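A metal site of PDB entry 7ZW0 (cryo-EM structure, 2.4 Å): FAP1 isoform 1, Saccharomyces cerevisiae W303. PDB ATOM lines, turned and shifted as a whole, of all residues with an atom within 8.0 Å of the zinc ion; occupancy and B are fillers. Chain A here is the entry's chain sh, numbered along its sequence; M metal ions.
The zinc ion is bound by SG of Cys 330, SG of Cys 371, SG of Cys 328 and SG of Cys 352. The zinc ion has four donor atoms within binding distance.
Merely in contact with the zinc ion: Ser 354 (3.96 Å). Along chain A the residues within 4 Å of the zinc ion span positions 328 to 371.
The backbone carbonyl oxygen (O) of Ser 354 is in hydrogen-bond range of the backbone NH (N) of Cys 371 (3.0 Å). O of Pro 350 lies close to SG of Cys 328 (3.7 Å). N of Cys 328 is in hydrogen-bond range of O of Thr 333, at 3.4 Å. The side-chain sulfur of Cys 352 lies close to the backbone NH of Ser 354 (3.5 Å).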
ATOM      1  N   THR A 327     -20.370 -16.374  -0.331  1.00  0.00           N
ATOM      2  CA  THR A 327     -19.316 -16.867   0.552  1.00  0.00           C
ATOM      3  C   THR A 327     -18.680 -15.720   1.324  1.00  0.00           C
ATOM      4  O   THR A 327     -18.963 -14.559   1.048  1.00  0.00           O
ATOM      5  CB  THR A 327     -18.213 -17.627  -0.204  1.00  0.00           C
ATOM      6  OG1 THR A 327     -17.483 -16.724  -1.033  1.00  0.00           O
ATOM      7  CG2 THR A 327     -18.804 -18.741  -1.048  1.00  0.00           C
ATOM      8  N   CYS A 328     -17.852 -16.056   2.299  1.00  0.00           N
ATOM      9  CA  CYS A 328     -17.203 -15.033   3.125  1.00  0.00           C
ATOM     10  C   CYS A 328     -16.120 -14.337   2.307  1.00  0.00           C
ATOM     11  O   CYS A 328     -15.741 -14.823   1.248  1.00  0.00           O
ATOM     12  CB  CYS A 328     -16.575 -15.716   4.340  1.00  0.00           C
ATOM     13  SG  CYS A 328     -16.689 -14.834   5.914  1.00  0.00           S
ATOM     14  N   PRO A 329     -15.635 -13.181   2.780  1.00  0.00           N
ATOM     15  CA  PRO A 329     -14.520 -12.566   2.049  1.00  0.00           C
ATOM     16  C   PRO A 329     -13.348 -13.531   2.092  1.00  0.00           C
ATOM     17  O   PRO A 329     -12.639 -13.686   1.099  1.00  0.00           O
ATOM     18  CB  PRO A 329     -14.183 -11.330   2.869  1.00  0.00           C
ATOM     19  CG  PRO A 329     -15.458 -10.973   3.555  1.00  0.00           C
ATOM     20  CD  PRO A 329     -16.256 -12.229   3.722  1.00  0.00           C
ATOM     21  N   CYS A 330     -13.132 -14.175   3.243  1.00  0.00           N
ATOM     22  CA  CYS A 330     -12.068 -15.150   3.358  1.00  0.00           C
ATOM     23  C   CYS A 330     -12.369 -16.388   2.533  1.00  0.00           C
ATOM     24  O   CYS A 330     -11.495 -17.224   2.333  1.00  0.00           O
ATOM     25  CB  CYS A 330     -11.888 -15.562   4.824  1.00  0.00           C
ATOM     26  SG  CYS A 330     -13.193 -16.608   5.500  1.00  0.00           S
ATOM     27  N   GLY A 331     -13.604 -16.510   2.038  1.00  0.00           N
ATOM     28  CA  GLY A 331     -13.963 -17.712   1.320  1.00  0.00           C
ATOM     29  C   GLY A 331     -14.005 -18.780   2.383  1.00  0.00           C
ATOM     30  O   GLY A 331     -14.688 -18.579   3.382  1.00  0.00           O
ATOM     31  N   ARG A 332     -13.311 -19.888   2.173  1.00  0.00           N
ATOM     32  CA  ARG A 332     -13.278 -20.994   3.141  1.00  0.00           C
ATOM     33  C   ARG A 332     -14.658 -21.617   3.392  1.00  0.00           C
ATOM     34  O   ARG A 332     -14.881 -22.769   3.028  1.00  0.00           O
ATOM     35  CB  ARG A 332     -12.585 -20.586   4.447  1.00  0.00           C
ATOM     36  CG  ARG A 332     -11.151 -20.118   4.257  1.00  0.00           C
ATOM     37  CD  ARG A 332     -10.427 -19.947   5.579  1.00  0.00           C
ATOM     38  NE  ARG A 332      -9.070 -19.439   5.381  1.00  0.00           N
ATOM     39  CZ  ARG A 332      -8.150 -19.337   6.333  1.00  0.00           C
ATOM     40  NH1 ARG A 332      -8.430 -19.708   7.575  1.00  0.00           N
ATOM     41  NH2 ARG A 332      -6.945 -18.856   6.053  1.00  0.00           N
ATOM     42  N   THR A 333     -15.580 -20.872   4.010  1.00  0.00           N
ATOM     43  CA  THR A 333     -16.924 -21.406   4.194  1.00  0.00           C
ATOM     44  C   THR A 333     -17.955 -20.449   3.613  1.00  0.00           C
ATOM     45  O   THR A 333     -17.676 -19.261   3.450  1.00  0.00           O
ATOM     46  CB  THR A 333     -17.236 -21.631   5.697  1.00  0.00           C
ATOM     47  OG1 THR A 333     -16.016 -21.815   6.422  1.00  0.00           O
ATOM     48  CG2 THR A 333     -18.132 -22.848   5.887  1.00  0.00           C
ATOM     49  N   LEU A 335     -20.872 -17.860   3.352  1.00  0.00           N
ATOM     50  CA  LEU A 335     -21.213 -16.781   4.284  1.00  0.00           C
ATOM     51  C   LEU A 335     -22.493 -17.064   5.041  1.00  0.00           C
ATOM     52  O   LEU A 335     -22.556 -16.833   6.243  1.00  0.00           O
ATOM     53  CB  LEU A 335     -21.336 -15.466   3.517  1.00  0.00           C
ATOM     54  CG  LEU A 335     -21.296 -14.135   4.268  1.00  0.00           C
ATOM     55  CD1 LEU A 335     -22.678 -13.656   4.674  1.00  0.00           C
ATOM     56  CD2 LEU A 335     -20.351 -14.206   5.463  1.00  0.00           C
ATOM     57  N   LEU A 338     -22.010 -19.420   8.004  1.00  0.00           N
ATOM     58  CA  LEU A 338     -21.301 -18.768   9.102  1.00  0.00           C
ATOM     59  C   LEU A 338     -22.146 -17.776   9.877  1.00  0.00           C
ATOM     60  O   LEU A 338     -22.141 -17.770  11.105  1.00  0.00           O
ATOM     61  CB  LEU A 338     -20.060 -18.049   8.560  1.00  0.00           C
ATOM     62  CG  LEU A 338     -18.988 -18.944   7.941  1.00  0.00           C
ATOM     63  CD1 LEU A 338     -18.086 -18.121   7.038  1.00  0.00           C
ATOM     64  CD2 LEU A 338     -18.193 -19.661   9.012  1.00  0.00           C
ATOM     65  N   ILE A 349     -20.000  -7.163   5.030  1.00  0.00           N
ATOM     66  CA  ILE A 349     -20.096  -8.612   5.032  1.00  0.00           C
ATOM     67  C   ILE A 349     -19.744  -9.127   6.414  1.00  0.00           C
ATOM     68  O   ILE A 349     -18.799  -8.624   7.033  1.00  0.00           O
ATOM     69  CB  ILE A 349     -19.116  -9.235   4.031  1.00  0.00           C
ATOM     70  CG1 ILE A 349     -18.954  -8.337   2.809  1.00  0.00           C
ATOM     71  CG2 ILE A 349     -19.550 -10.630   3.615  1.00  0.00           C
ATOM     72  CD1 ILE A 349     -17.797  -8.744   1.922  1.00  0.00           C
ATOM     73  N   PRO A 350     -20.515 -10.110   6.971  1.00  0.00           N
ATOM     74  CA  PRO A 350     -20.090 -10.538   8.310  1.00  0.00           C
ATOM     75  C   PRO A 350     -18.675 -11.090   8.398  1.00  0.00           C
ATOM     76  O   PRO A 350     -18.358 -12.081   7.723  1.00  0.00           O
ATOM     77  CB  PRO A 350     -21.099 -11.635   8.661  1.00  0.00           C
ATOM     78  CG  PRO A 350     -22.332 -11.223   7.940  1.00  0.00           C
ATOM     79  CD  PRO A 350     -21.824 -10.704   6.624  1.00  0.00           C
ATOM     80  N   THR A 351     -17.848 -10.493   9.256  1.00  0.00           N
ATOM     81  CA  THR A 351     -16.492 -10.972   9.448  1.00  0.00           C
ATOM     82  C   THR A 351     -16.503 -12.296  10.199  1.00  0.00           C
ATOM     83  O   THR A 351     -17.401 -12.552  11.006  1.00  0.00           O
ATOM     84  CB  THR A 351     -15.686  -9.954  10.272  1.00  0.00           C
ATOM     85  OG1 THR A 351     -16.196  -9.898  11.610  1.00  0.00           O
ATOM     86  CG2 THR A 351     -15.785  -8.575   9.639  1.00  0.00           C
ATOM     87  N   CYS A 352     -15.511 -13.141   9.949  1.00  0.00           N
ATOM     88  CA  CYS A 352     -15.456 -14.447  10.609  1.00  0.00           C
ATOM     89  C   CYS A 352     -14.057 -14.712  11.136  1.00  0.00           C
ATOM     90  O   CYS A 352     -13.091 -14.092  10.697  1.00  0.00           O
ATOM     91  CB  CYS A 352     -15.917 -15.565   9.674  1.00  0.00           C
ATOM     92  SG  CYS A 352     -14.608 -16.321   8.680  1.00  0.00           S
ATOM     93  N   ASP A 353     -13.925 -15.655  12.070  1.00  0.00           N
ATOM     94  CA  ASP A 353     -12.629 -15.929  12.686  1.00  0.00           C
ATOM     95  C   ASP A 353     -11.566 -16.388  11.700  1.00  0.00           C
ATOM     96  O   ASP A 353     -10.403 -16.010  11.838  1.00  0.00           O
ATOM     97  CB  ASP A 353     -12.781 -16.955  13.806  1.00  0.00           C
ATOM     98  CG  ASP A 353     -13.575 -16.431  14.985  1.00  0.00           C
ATOM     99  OD1 ASP A 353     -13.924 -15.226  14.977  1.00  0.00           O
ATOM    100  OD2 ASP A 353     -13.848 -17.216  15.918  1.00  0.00           O
ATOM    101  N   SER A 354     -11.940 -17.182  10.705  1.00  0.00           N
ATOM    102  CA  SER A 354     -10.959 -17.709   9.769  1.00  0.00           C
ATOM    103  C   SER A 354     -10.236 -16.601   9.023  1.00  0.00           C
ATOM    104  O   SER A 354     -10.843 -15.587   8.676  1.00  0.00           O
ATOM    105  CB  SER A 354     -11.636 -18.645   8.768  1.00  0.00           C
ATOM    106  OG  SER A 354     -12.238 -19.746   9.437  1.00  0.00           O
ATOM    107  N   ARG A 355      -8.939 -16.778   8.772  1.00  0.00           N
ATOM    108  CA  ARG A 355      -8.151 -15.720   8.149  1.00  0.00           C
ATOM    109  C   ARG A 355      -8.609 -15.331   6.750  1.00  0.00           C
ATOM    110  O   ARG A 355      -8.929 -16.195   5.931  1.00  0.00           O
ATOM    111  CB  ARG A 355      -6.688 -16.145   8.089  1.00  0.00           C
ATOM    112  CG  ARG A 355      -6.247 -16.938   9.312  1.00  0.00           C
ATOM    113  CD  ARG A 355      -4.774 -17.308   9.269  1.00  0.00           C
ATOM    114  NE  ARG A 355      -4.246 -17.468  10.620  1.00  0.00           N
ATOM    115  CZ  ARG A 355      -2.977 -17.755  10.887  1.00  0.00           C
ATOM    116  NH1 ARG A 355      -2.101 -17.927   9.908  1.00  0.00           N
ATOM    117  NH2 ARG A 355      -2.579 -17.875  12.155  1.00  0.00           N
ATOM    118  N   CYS A 356      -8.630 -14.026   6.469  1.00  0.00           N
ATOM    119  CA  CYS A 356      -9.089 -13.558   5.162  1.00  0.00           C
ATOM    120  C   CYS A 356      -8.178 -13.983   4.027  1.00  0.00           C
ATOM    121  O   CYS A 356      -8.653 -14.338   2.950  1.00  0.00           O
ATOM    122  CB  CYS A 356      -9.290 -12.040   5.154  1.00  0.00           C
ATOM    123  SG  CYS A 356      -8.544 -11.205   6.566  1.00  0.00           S
ATOM    124  N   GLY A 357      -6.863 -13.945   4.252  1.00  0.00           N
ATOM    125  CA  GLY A 357      -5.936 -14.398   3.237  1.00  0.00           C
ATOM    126  C   GLY A 357      -5.920 -13.455   2.047  1.00  0.00           C
ATOM    127  O   GLY A 357      -5.464 -13.822   0.965  1.00  0.00           O
ATOM    128  N   LYS A 358      -6.415 -12.240   2.244  1.00  0.00           N
ATOM    129  CA  LYS A 358      -6.425 -11.264   1.170  1.00  0.00           C
ATOM    130  C   LYS A 358      -5.015 -10.880   0.764  1.00  0.00           C
ATOM    131  O   LYS A 358      -4.160 -10.656   1.618  1.00  0.00           O
ATOM    132  CB  LYS A 358      -7.222 -10.012   1.585  1.00  0.00           C
ATOM    133  CG  LYS A 358      -8.702 -10.270   1.730  1.00  0.00           C
ATOM    134  CD  LYS A 358      -9.477  -8.982   1.971  1.00  0.00           C
ATOM    135  CE  LYS A 358     -10.972  -9.256   2.006  1.00  0.00           C
ATOM    136  NZ  LYS A 358     -11.779  -8.003   2.071  1.00  0.00           N
ATOM    137  N   PHE A 369      -4.639 -12.199   9.312  1.00  0.00           N
ATOM    138  CA  PHE A 369      -5.596 -11.496  10.159  1.00  0.00           C
ATOM    139  C   PHE A 369      -6.956 -12.185  10.104  1.00  0.00           C
ATOM    140  O   PHE A 369      -7.283 -12.835   9.119  1.00  0.00           O
ATOM    141  CB  PHE A 369      -5.759 -10.055   9.694  1.00  0.00           C
ATOM    142  CG  PHE A 369      -4.466  -9.322   9.529  1.00  0.00           C
ATOM    143  CD1 PHE A 369      -3.880  -8.659  10.587  1.00  0.00           C
ATOM    144  CD2 PHE A 369      -3.835  -9.279   8.296  1.00  0.00           C
ATOM    145  CE1 PHE A 369      -2.693  -7.978  10.431  1.00  0.00           C
ATOM    146  CE2 PHE A 369      -2.645  -8.598   8.126  1.00  0.00           C
ATOM    147  CZ  PHE A 369      -2.071  -7.946   9.202  1.00  0.00           C
ATOM    148  N   THR A 370      -7.761 -12.020  11.146  1.00  0.00           N
ATOM    149  CA  THR A 370      -9.114 -12.588  11.153  1.00  0.00           C
ATOM    150  C   THR A 370      -9.871 -11.923  10.018  1.00  0.00           C
ATOM    151  O   THR A 370      -9.649 -10.742   9.728  1.00  0.00           O
ATOM    152  CB  THR A 370      -9.789 -12.404  12.528  1.00  0.00           C
ATOM    153  OG1 THR A 370      -9.581 -13.579  13.328  1.00  0.00           O
ATOM    154  CG2 THR A 370     -11.281 -12.163  12.423  1.00  0.00           C
ATOM    155  N   CYS A 371     -10.788 -12.640   9.365  1.00  0.00           N
ATOM    156  CA  CYS A 371     -11.448 -12.089   8.183  1.00  0.00           C
ATOM    157  C   CYS A 371     -12.115 -10.754   8.378  1.00  0.00           C
ATOM    158  O   CYS A 371     -12.752 -10.515   9.402  1.00  0.00           O
ATOM    159  CB  CYS A 371     -12.484 -13.091   7.652  1.00  0.00           C
ATOM    160  SG  CYS A 371     -13.665 -12.400   6.472  1.00  0.00           S
ATOM    161  N   HIS A 372     -11.943  -9.861   7.410  1.00  0.00           N
ATOM    162  CA  HIS A 372     -12.581  -8.557   7.476  1.00  0.00           C
ATOM    163  C   HIS A 372     -13.197  -8.233   6.122  1.00  0.00           C
ATOM    164  O   HIS A 372     -12.675  -8.646   5.090  1.00  0.00           O
ATOM    165  CB  HIS A 372     -11.575  -7.479   7.883  1.00  0.00           C
ATOM    166  CG  HIS A 372     -10.202  -7.672   7.304  1.00  0.00           C
ATOM    167  ND1 HIS A 372      -9.919  -7.492   5.978  1.00  0.00           N
ATOM    168  CD2 HIS A 372      -9.031  -8.010   7.899  1.00  0.00           C
ATOM    169  CE1 HIS A 372      -8.637  -7.721   5.761  1.00  0.00           C
ATOM    170  NE2 HIS A 372      -8.077  -8.043   6.908  1.00  0.00           N
ATOM    171  N   ASP A 373     -14.313  -7.513   6.130  1.00  0.00           N
ATOM    172  CA  ASP A 373     -15.009  -7.190   4.888  1.00  0.00           C
ATOM    173  C   ASP A 373     -14.173  -6.234   4.050  1.00  0.00           C
ATOM    174  O   ASP A 373     -14.135  -6.339   2.828  1.00  0.00           O
ATOM    175  CB  ASP A 373     -16.381  -6.598   5.178  1.00  0.00           C
ATOM    176  CG  ASP A 373     -16.333  -5.461   6.180  1.00  0.00           C
ATOM    177  OD1 ASP A 373     -16.330  -5.732   7.394  1.00  0.00           O
ATOM    178  OD2 ASP A 373     -16.306  -4.291   5.753  1.00  0.00           O
HETATM  179 ZN    ZN M   1     -13.989 -14.832   6.396  1.00  0.00          ZN
